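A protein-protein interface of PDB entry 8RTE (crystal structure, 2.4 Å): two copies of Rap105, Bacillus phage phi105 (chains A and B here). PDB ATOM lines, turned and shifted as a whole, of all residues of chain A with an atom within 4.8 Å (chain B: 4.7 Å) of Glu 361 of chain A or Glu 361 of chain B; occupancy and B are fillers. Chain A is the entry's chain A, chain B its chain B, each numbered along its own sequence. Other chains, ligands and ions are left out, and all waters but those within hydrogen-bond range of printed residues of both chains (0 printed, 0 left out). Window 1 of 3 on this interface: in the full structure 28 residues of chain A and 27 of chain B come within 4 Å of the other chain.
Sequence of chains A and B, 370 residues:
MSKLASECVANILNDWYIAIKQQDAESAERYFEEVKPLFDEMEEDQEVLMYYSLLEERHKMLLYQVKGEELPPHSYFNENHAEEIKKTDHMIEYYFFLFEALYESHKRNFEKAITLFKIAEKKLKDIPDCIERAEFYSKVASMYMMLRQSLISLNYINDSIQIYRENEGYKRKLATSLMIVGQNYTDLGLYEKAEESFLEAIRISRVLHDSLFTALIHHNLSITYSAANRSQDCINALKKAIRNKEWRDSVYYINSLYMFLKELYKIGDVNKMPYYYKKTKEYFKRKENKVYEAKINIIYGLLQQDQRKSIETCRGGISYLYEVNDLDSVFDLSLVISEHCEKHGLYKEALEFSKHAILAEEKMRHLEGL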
ATOM      1  N   ARG A 148      -5.100  23.984  28.764  1.00  0.00           N
ATOM      2  CA  ARG A 148      -3.872  24.745  28.990  1.00  0.00           C
ATOM      3  C   ARG A 148      -4.169  26.231  29.184  1.00  0.00           C
ATOM      4  O   ARG A 148      -3.341  27.090  28.874  1.00  0.00           O
ATOM      5  CB  ARG A 148      -2.882  24.517  27.842  1.00  0.00           C
ATOM      6  CG  ARG A 148      -2.370  23.081  27.778  1.00  0.00           C
ATOM      7  CD  ARG A 148      -1.164  22.925  26.868  1.00  0.00           C
ATOM      8  NE  ARG A 148      -0.033  23.767  27.235  1.00  0.00           N
ATOM      9  CZ  ARG A 148       0.781  24.330  26.351  1.00  0.00           C
ATOM     10  NH1 ARG A 148       0.563  24.229  25.049  1.00  0.00           N
ATOM     11  NH2 ARG A 148       1.831  25.024  26.782  1.00  0.00           N
ATOM     12  N   PHE A 331      -0.980  17.984  19.879  1.00  0.00           N
ATOM     13  CA  PHE A 331       0.146  18.894  20.083  1.00  0.00           C
ATOM     14  C   PHE A 331       1.377  18.151  20.585  1.00  0.00           C
ATOM     15  O   PHE A 331       2.480  18.319  20.049  1.00  0.00           O
ATOM     16  CB  PHE A 331      -0.251  19.993  21.066  1.00  0.00           C
ATOM     17  CG  PHE A 331       0.870  20.939  21.410  1.00  0.00           C
ATOM     18  CD1 PHE A 331       1.253  21.930  20.522  1.00  0.00           C
ATOM     19  CD2 PHE A 331       1.529  20.844  22.625  1.00  0.00           C
ATOM     20  CE1 PHE A 331       2.277  22.805  20.834  1.00  0.00           C
ATOM     21  CE2 PHE A 331       2.554  21.715  22.944  1.00  0.00           C
ATOM     22  CZ  PHE A 331       2.929  22.696  22.048  1.00  0.00           C
ATOM     23  N   ALA A 357       1.086  20.500  15.048  1.00  0.00           N
ATOM     24  CA  ALA A 357       1.273  20.973  16.415  1.00  0.00           C
ATOM     25  C   ALA A 357       0.752  22.395  16.584  1.00  0.00           C
ATOM     26  O   ALA A 357       0.141  22.721  17.609  1.00  0.00           O
ATOM     27  CB  ALA A 357       2.747  20.889  16.814  1.00  0.00           C
ATOM     28  N   ILE A 358       1.002  23.262  15.600  1.00  0.00           N
ATOM     29  CA  ILE A 358       0.466  24.621  15.641  1.00  0.00           C
ATOM     30  C   ILE A 358      -1.056  24.600  15.579  1.00  0.00           C
ATOM     31  O   ILE A 358      -1.735  25.278  16.359  1.00  0.00           O
ATOM     32  CB  ILE A 358       1.064  25.475  14.510  1.00  0.00           C
ATOM     33  CG1 ILE A 358       2.556  25.713  14.757  1.00  0.00           C
ATOM     34  CG2 ILE A 358       0.315  26.788  14.390  1.00  0.00           C
ATOM     35  CD1 ILE A 358       3.328  26.081  13.509  1.00  0.00           C
ATOM     36  N   LEU A 359      -1.611  23.839  14.633  1.00  0.00           N
ATOM     37  CA  LEU A 359      -3.064  23.764  14.488  1.00  0.00           C
ATOM     38  C   LEU A 359      -3.733  23.307  15.781  1.00  0.00           C
ATOM     39  O   LEU A 359      -4.693  23.928  16.252  1.00  0.00           O
ATOM     40  CB  LEU A 359      -3.428  22.825  13.339  1.00  0.00           C
ATOM     41  CG  LEU A 359      -3.133  23.293  11.917  1.00  0.00           C
ATOM     42  CD1 LEU A 359      -3.489  22.200  10.919  1.00  0.00           C
ATOM     43  CD2 LEU A 359      -3.879  24.586  11.608  1.00  0.00           C
ATOM     44  N   ALA A 360      -3.253  22.199  16.354  1.00  0.00           N
ATOM     45  CA  ALA A 360      -3.815  21.703  17.609  1.00  0.00           C
ATOM     46  C   ALA A 360      -3.732  22.748  18.714  1.00  0.00           C
ATOM     47  O   ALA A 360      -4.675  22.910  19.497  1.00  0.00           O
ATOM     48  CB  ALA A 360      -3.101  20.425  18.036  1.00  0.00           C
ATOM     49  N   GLU A 361      -2.608  23.456  18.803  1.00  0.00           N
ATOM     50  CA  GLU A 361      -2.420  24.413  19.884  1.00  0.00           C
ATOM     51  C   GLU A 361      -3.295  25.645  19.678  1.00  0.00           C
ATOM     52  O   GLU A 361      -3.862  26.173  20.643  1.00  0.00           O
ATOM     53  CB  GLU A 361      -0.931  24.766  20.002  1.00  0.00           C
ATOM     54  CG  GLU A 361      -0.577  25.763  21.094  1.00  0.00           C
ATOM     55  CD  GLU A 361      -0.657  27.200  20.623  1.00  0.00           C
ATOM     56  OE1 GLU A 361      -0.191  27.478  19.494  1.00  0.00           O
ATOM     57  OE2 GLU A 361      -1.178  28.046  21.376  1.00  0.00           O
ATOM     58  N   GLU A 362      -3.408  26.126  18.433  1.00  0.00           N
ATOM     59  CA  GLU A 362      -4.271  27.275  18.169  1.00  0.00           C
ATOM     60  C   GLU A 362      -5.737  26.935  18.404  1.00  0.00           C
ATOM     61  O   GLU A 362      -6.483  27.749  18.957  1.00  0.00           O
ATOM     62  CB  GLU A 362      -4.072  27.781  16.743  1.00  0.00           C
ATOM     63  CG  GLU A 362      -2.739  28.485  16.521  1.00  0.00           C
ATOM     64  CD  GLU A 362      -2.496  29.604  17.522  1.00  0.00           C
ATOM     65  OE1 GLU A 362      -3.167  30.661  17.438  1.00  0.00           O
ATOM     66  OE2 GLU A 362      -1.625  29.429  18.395  1.00  0.00           O
ATOM     67  N   LYS A 363      -6.176  25.745  17.979  1.00  0.00           N
ATOM     68  CA  LYS A 363      -7.559  25.342  18.235  1.00  0.00           C
ATOM     69  C   LYS A 363      -7.800  25.131  19.727  1.00  0.00           C
ATOM     70  O   LYS A 363      -8.880  25.452  20.237  1.00  0.00           O
ATOM     71  CB  LYS A 363      -7.899  24.083  17.434  1.00  0.00           C
ATOM     72  CG  LYS A 363      -9.378  23.711  17.427  1.00  0.00           C
ATOM     73  N   MET A 364      -6.806  24.583  20.441  1.00  0.00           N
ATOM     74  CA  MET A 364      -6.920  24.437  21.891  1.00  0.00           C
ATOM     75  C   MET A 364      -7.100  25.792  22.562  1.00  0.00           C
ATOM     76  O   MET A 364      -7.834  25.920  23.550  1.00  0.00           O
ATOM     77  CB  MET A 364      -5.687  23.727  22.453  1.00  0.00           C
ATOM     78  CG  MET A 364      -5.974  22.829  23.650  1.00  0.00           C
ATOM     79  SD  MET A 364      -4.447  22.179  24.348  1.00  0.00           S
ATOM     80  CE  MET A 364      -3.507  21.903  22.849  1.00  0.00           C
ATOM     81  N   ARG A 365      -6.426  26.813  22.044  1.00  0.00           N
ATOM     82  CA  ARG A 365      -6.520  28.145  22.619  1.00  0.00           C
ATOM     83  C   ARG A 365      -7.815  28.838  22.212  1.00  0.00           C
ATOM     84  O   ARG A 365      -8.220  29.822  22.843  1.00  0.00           O
ATOM     85  CB  ARG A 365      -5.299  28.964  22.162  1.00  0.00           C
ATOM     86  CG  ARG A 365      -5.371  30.469  22.332  1.00  0.00           C
ATOM     87  CD  ARG A 365      -4.384  31.169  21.408  1.00  0.00           C
ATOM     88  NE  ARG A 365      -3.015  30.735  21.653  1.00  0.00           N
ATOM     89  CZ  ARG A 365      -2.201  31.293  22.539  1.00  0.00           C
ATOM     90  NH1 ARG A 365      -2.593  32.302  23.300  1.00  0.00           N
ATOM     91  NH2 ARG A 365      -0.967  30.812  22.682  1.00  0.00           N
ATOM     92  N   ARG B 148      -1.600  37.626  24.345  1.00  0.00           N
ATOM     93  CA  ARG B 148      -2.673  36.716  23.933  1.00  0.00           C
ATOM     94  C   ARG B 148      -3.201  35.909  25.115  1.00  0.00           C
ATOM     95  O   ARG B 148      -3.646  34.774  24.966  1.00  0.00           O
ATOM     96  CB  ARG B 148      -2.256  35.802  22.773  1.00  0.00           C
ATOM     97  CG  ARG B 148      -2.019  36.577  21.479  1.00  0.00           C
ATOM     98  CD  ARG B 148      -2.130  35.728  20.210  1.00  0.00           C
ATOM     99  NE  ARG B 148      -1.498  34.416  20.286  1.00  0.00           N
ATOM    100  CZ  ARG B 148      -1.854  33.385  19.531  1.00  0.00           C
ATOM    101  NH1 ARG B 148      -2.808  33.493  18.616  1.00  0.00           N
ATOM    102  NH2 ARG B 148      -1.229  32.222  19.683  1.00  0.00           N
ATOM    103  N   PHE B 331       5.878  34.856  15.920  1.00  0.00           N
ATOM    104  CA  PHE B 331       4.851  33.862  15.627  1.00  0.00           C
ATOM    105  C   PHE B 331       4.180  34.136  14.288  1.00  0.00           C
ATOM    106  O   PHE B 331       4.049  33.233  13.453  1.00  0.00           O
ATOM    107  CB  PHE B 331       3.815  33.831  16.745  1.00  0.00           C
ATOM    108  CG  PHE B 331       2.658  32.920  16.464  1.00  0.00           C
ATOM    109  CD1 PHE B 331       2.787  31.548  16.602  1.00  0.00           C
ATOM    110  CD2 PHE B 331       1.437  33.439  16.060  1.00  0.00           C
ATOM    111  CE1 PHE B 331       1.719  30.709  16.339  1.00  0.00           C
ATOM    112  CE2 PHE B 331       0.372  32.610  15.797  1.00  0.00           C
ATOM    113  CZ  PHE B 331       0.510  31.243  15.936  1.00  0.00           C
ATOM    114  N   ALA B 357       7.868  29.554  15.197  1.00  0.00           N
ATOM    115  CA  ALA B 357       6.509  29.944  15.561  1.00  0.00           C
ATOM    116  C   ALA B 357       6.059  29.236  16.837  1.00  0.00           C
ATOM    117  O   ALA B 357       5.414  29.848  17.696  1.00  0.00           O
ATOM    118  CB  ALA B 357       5.553  29.655  14.405  1.00  0.00           C
ATOM    119  N   ILE B 358       6.387  27.948  16.973  1.00  0.00           N
ATOM    120  CA  ILE B 358       6.089  27.223  18.206  1.00  0.00           C
ATOM    121  C   ILE B 358       6.864  27.822  19.373  1.00  0.00           C
ATOM    122  O   ILE B 358       6.299  28.108  20.435  1.00  0.00           O
ATOM    123  CB  ILE B 358       6.396  25.724  18.035  1.00  0.00           C
ATOM    124  CG1 ILE B 358       5.438  25.100  17.020  1.00  0.00           C
ATOM    125  CG2 ILE B 358       6.286  24.987  19.370  1.00  0.00           C
ATOM    126  CD1 ILE B 358       5.964  23.826  16.406  1.00  0.00           C
ATOM    127  N   LEU B 359       8.170  28.021  19.191  1.00  0.00           N
ATOM    128  CA  LEU B 359       8.998  28.590  20.253  1.00  0.00           C
ATOM    129  C   LEU B 359       8.476  29.953  20.691  1.00  0.00           C
ATOM    130  O   LEU B 359       8.340  30.224  21.891  1.00  0.00           O
ATOM    131  CB  LEU B 359      10.450  28.689  19.795  1.00  0.00           C
ATOM    132  CG  LEU B 359      11.456  28.912  20.924  1.00  0.00           C
ATOM    133  CD1 LEU B 359      11.239  27.892  22.028  1.00  0.00           C
ATOM    134  CD2 LEU B 359      12.863  28.817  20.375  1.00  0.00           C
ATOM    135  N   ALA B 360       8.212  30.840  19.726  1.00  0.00           N
ATOM    136  CA  ALA B 360       7.667  32.155  20.051  1.00  0.00           C
ATOM    137  C   ALA B 360       6.369  32.040  20.840  1.00  0.00           C
ATOM    138  O   ALA B 360       6.148  32.786  21.801  1.00  0.00           O
ATOM    139  CB  ALA B 360       7.445  32.964  18.776  1.00  0.00           C
ATOM    140  N   GLU B 361       5.497  31.107  20.452  1.00  0.00           N
ATOM    141  CA  GLU B 361       4.202  30.995  21.112  1.00  0.00           C
ATOM    142  C   GLU B 361       4.340  30.419  22.517  1.00  0.00           C
ATOM    143  O   GLU B 361       3.728  30.924  23.466  1.00  0.00           O
ATOM    144  CB  GLU B 361       3.269  30.133  20.269  1.00  0.00           C
ATOM    145  CG  GLU B 361       1.913  29.889  20.899  1.00  0.00           C
ATOM    146  CD  GLU B 361       1.929  28.707  21.846  1.00  0.00           C
ATOM    147  OE1 GLU B 361       2.550  27.675  21.503  1.00  0.00           O
ATOM    148  OE2 GLU B 361       1.339  28.814  22.942  1.00  0.00           O
ATOM    149  N   GLU B 362       5.145  29.363  22.669  1.00  0.00           N
ATOM    150  CA  GLU B 362       5.346  28.767  23.988  1.00  0.00           C
ATOM    151  C   GLU B 362       6.026  29.737  24.942  1.00  0.00           C
ATOM    152  O   GLU B 362       5.673  29.798  26.128  1.00  0.00           O
ATOM    153  CB  GLU B 362       6.157  27.479  23.863  1.00  0.00           C
ATOM    154  CG  GLU B 362       5.374  26.262  23.354  1.00  0.00           C
ATOM    155  CD  GLU B 362       4.176  25.913  24.235  1.00  0.00           C
ATOM    156  OE1 GLU B 362       4.404  25.415  25.361  1.00  0.00           O
ATOM    157  OE2 GLU B 362       3.021  26.109  23.806  1.00  0.00           O
ATOM    158  N   LYS B 363       7.002  30.505  24.445  1.00  0.00           N
ATOM    159  CA  LYS B 363       7.656  31.509  25.278  1.00  0.00           C
ATOM    160  C   LYS B 363       6.683  32.611  25.679  1.00  0.00           C
ATOM    161  O   LYS B 363       6.742  33.117  26.806  1.00  0.00           O
ATOM    162  CB  LYS B 363       8.856  32.109  24.545  1.00  0.00           C
ATOM    163  CG  LYS B 363      10.117  31.276  24.599  1.00  0.00           C
ATOM    164  CD  LYS B 363      11.227  31.905  23.763  1.00  0.00           C
ATOM    165  N   MET B 364       5.786  32.990  24.767  1.00  0.00           N
ATOM    166  CA  MET B 364       4.778  34.003  25.063  1.00  0.00           C
ATOM    167  C   MET B 364       3.880  33.584  26.222  1.00  0.00           C
ATOM    168  O   MET B 364       3.530  34.412  27.072  1.00  0.00           O
ATOM    169  CB  MET B 364       3.946  34.271  23.807  1.00  0.00           C
ATOM    170  CG  MET B 364       3.396  35.686  23.671  1.00  0.00           C
ATOM    171  SD  MET B 364       2.339  35.849  22.210  1.00  0.00           S
ATOM    172  CE  MET B 364       1.720  34.181  21.984  1.00  0.00           C
ATOM    173  N   ARG B 365       3.497  32.306  26.273  1.00  0.00           N
ATOM    174  CA  ARG B 365       2.588  31.793  27.301  1.00  0.00           C
ATOM    175  C   ARG B 365       3.276  31.438  28.619  1.00  0.00           C
ATOM    176  O   ARG B 365       2.579  31.080  29.579  1.00  0.00           O
ATOM    177  CB  ARG B 365       1.817  30.571  26.781  1.00  0.00           C
ATOM    178  CG  ARG B 365       2.522  29.245  26.964  1.00  0.00           C
ATOM    179  CD  ARG B 365       1.795  28.173  26.187  1.00  0.00           C
ATOM    180  NE  ARG B 365       0.392  28.102  26.574  1.00  0.00           N
ATOM    181  CZ  ARG B 365      -0.602  27.824  25.743  1.00  0.00           C
ATOM    182  NH1 ARG B 365      -0.383  27.584  24.459  1.00  0.00           N
ATOM    183  NH2 ARG B 365      -1.847  27.795  26.209  1.00  0.00           N
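Hydrophobic or aromatic side chains of chain A that line the printed part of chain B: Phe 331 and Ile 358.
Of the 11 printed residues of chain B, 6 touch a printed residue of chain A.
Among the printed residues, Asp or Glu carboxylates within 4 Å of a Lys or Arg side-chain nitrogen of the other chain: Arg 148 of chain A with Glu 362 of chain B (3.0 Å), Glu 361 of chain A with Arg 365 of chain B (3.2 Å), Glu 362 of chain A with Arg 148 of chain B (3.1 Å) and Arg 365 of chain A with Glu 361 of chain B (3.1 Å).
OE1 of Glu 361 of chain A sits close to OE2 of Glu 362 of chain A (2.7 Å).
OE2 of Glu 361 of chain A lies within salt-bridge range of NH2 of Arg 365 of chain A, at 3.1 Å.
NE of Arg 365 of chain A lies within salt-bridge range of OE2 of Glu 362 of chain A, 3.8 Å away.
The side-chain carboxylate (OE2) of Glu 361 of chain B lies within salt-bridge range of the guanidinium group (NH1) of Arg 365 of chain B.
The side-chain carboxylate (OE2) of Glu 362 of chain B lies within salt-bridge range of the guanidinium group (NH1) of Arg 365 of chain B (3.8 Å).
Glu 362 of chain B touches Phe 331 of chain A.
Ile 358 of chain A touches Ile 358 of chain B.
Phe 331 of chain B touches Glu 362 of chain A.
Arg 365 of chain A touches Arg 365 of chain B.
Of chain B, only Glu 361 (3.1 Å) and Arg 365 (3.2 Å) come within 4 Å of Glu 361 of chain A.
Of chain A, only Glu 361 and Arg 365 come within 4 Å of Glu 361 of chain B.
Of the printed residues of chain A, Arg 148 of chain B touches Glu 362 and Arg 365.
Of the printed residues of chain A, Phe 331 of chain B touches Glu 362 (3.7 Å).
Printed residues of chain B within 4 Å of Phe 331 of chain A: Glu 362 (3.8 Å).
Leu 359 of chain A touches none of the printed residues of chain B.
The nearest residue of chain A that does not touch Glu 361 of chain B is Glu 362 of chain A (4.4 Å).
Arg 148 of chain A touches Arg 365 of chain B, and with the chains exchanged Arg 365 of chain A touches Arg 148 of chain B.
Ile 358 of chain B touches its own counterpart, Ile 358 of chain A.
Glu 361 of chain B touches its own counterpart, Glu 361 of chain A.
Arg 365 of chain B touches its own counterpart, Arg 365 of chain A.
Positions printed for both chains: 148, 331, 357, 358, 359, 360, 361, 362, 363, 364 and 365.
Of the 11 pairs that touch across the chains among the printed residues, 11 have their exchanged pair printed and touching as well.
The guanidinium group (NH2) of Arg 148 of chain A is in salt-bridge range of the side-chain carboxylate (OE1) of Glu 362 of chain B (3.0 Å).
NH2 of Arg 365 of chain B sits at hydrogen-bond distance from O of Arg 148 of chain A, at 3.1 Å.
The guanidinium group of Arg 365 of chain B lies within salt-bridge range of the side-chain carboxylate of Glu 361 of chain A (3.2 Å).
The guanidinium group (NH1) of Arg 148 of chain B is in salt-bridge range of the side-chain carboxylate (OE1) of Glu 362 of chain A (3.1 Å).
The backbone carbonyl oxygen (O) of Arg 148 of chain B is in hydrogen-bond range of the guanidinium group (NH1) of Arg 365 of chain A, 3.2 Å away.
NH2 of Arg 365 of chain A is in salt-bridge range of OE2 of Glu 361 of chain B (3.1 Å).
OE2 of Glu 361 of chain A sits close to OE2 of Glu 361 of chain B.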
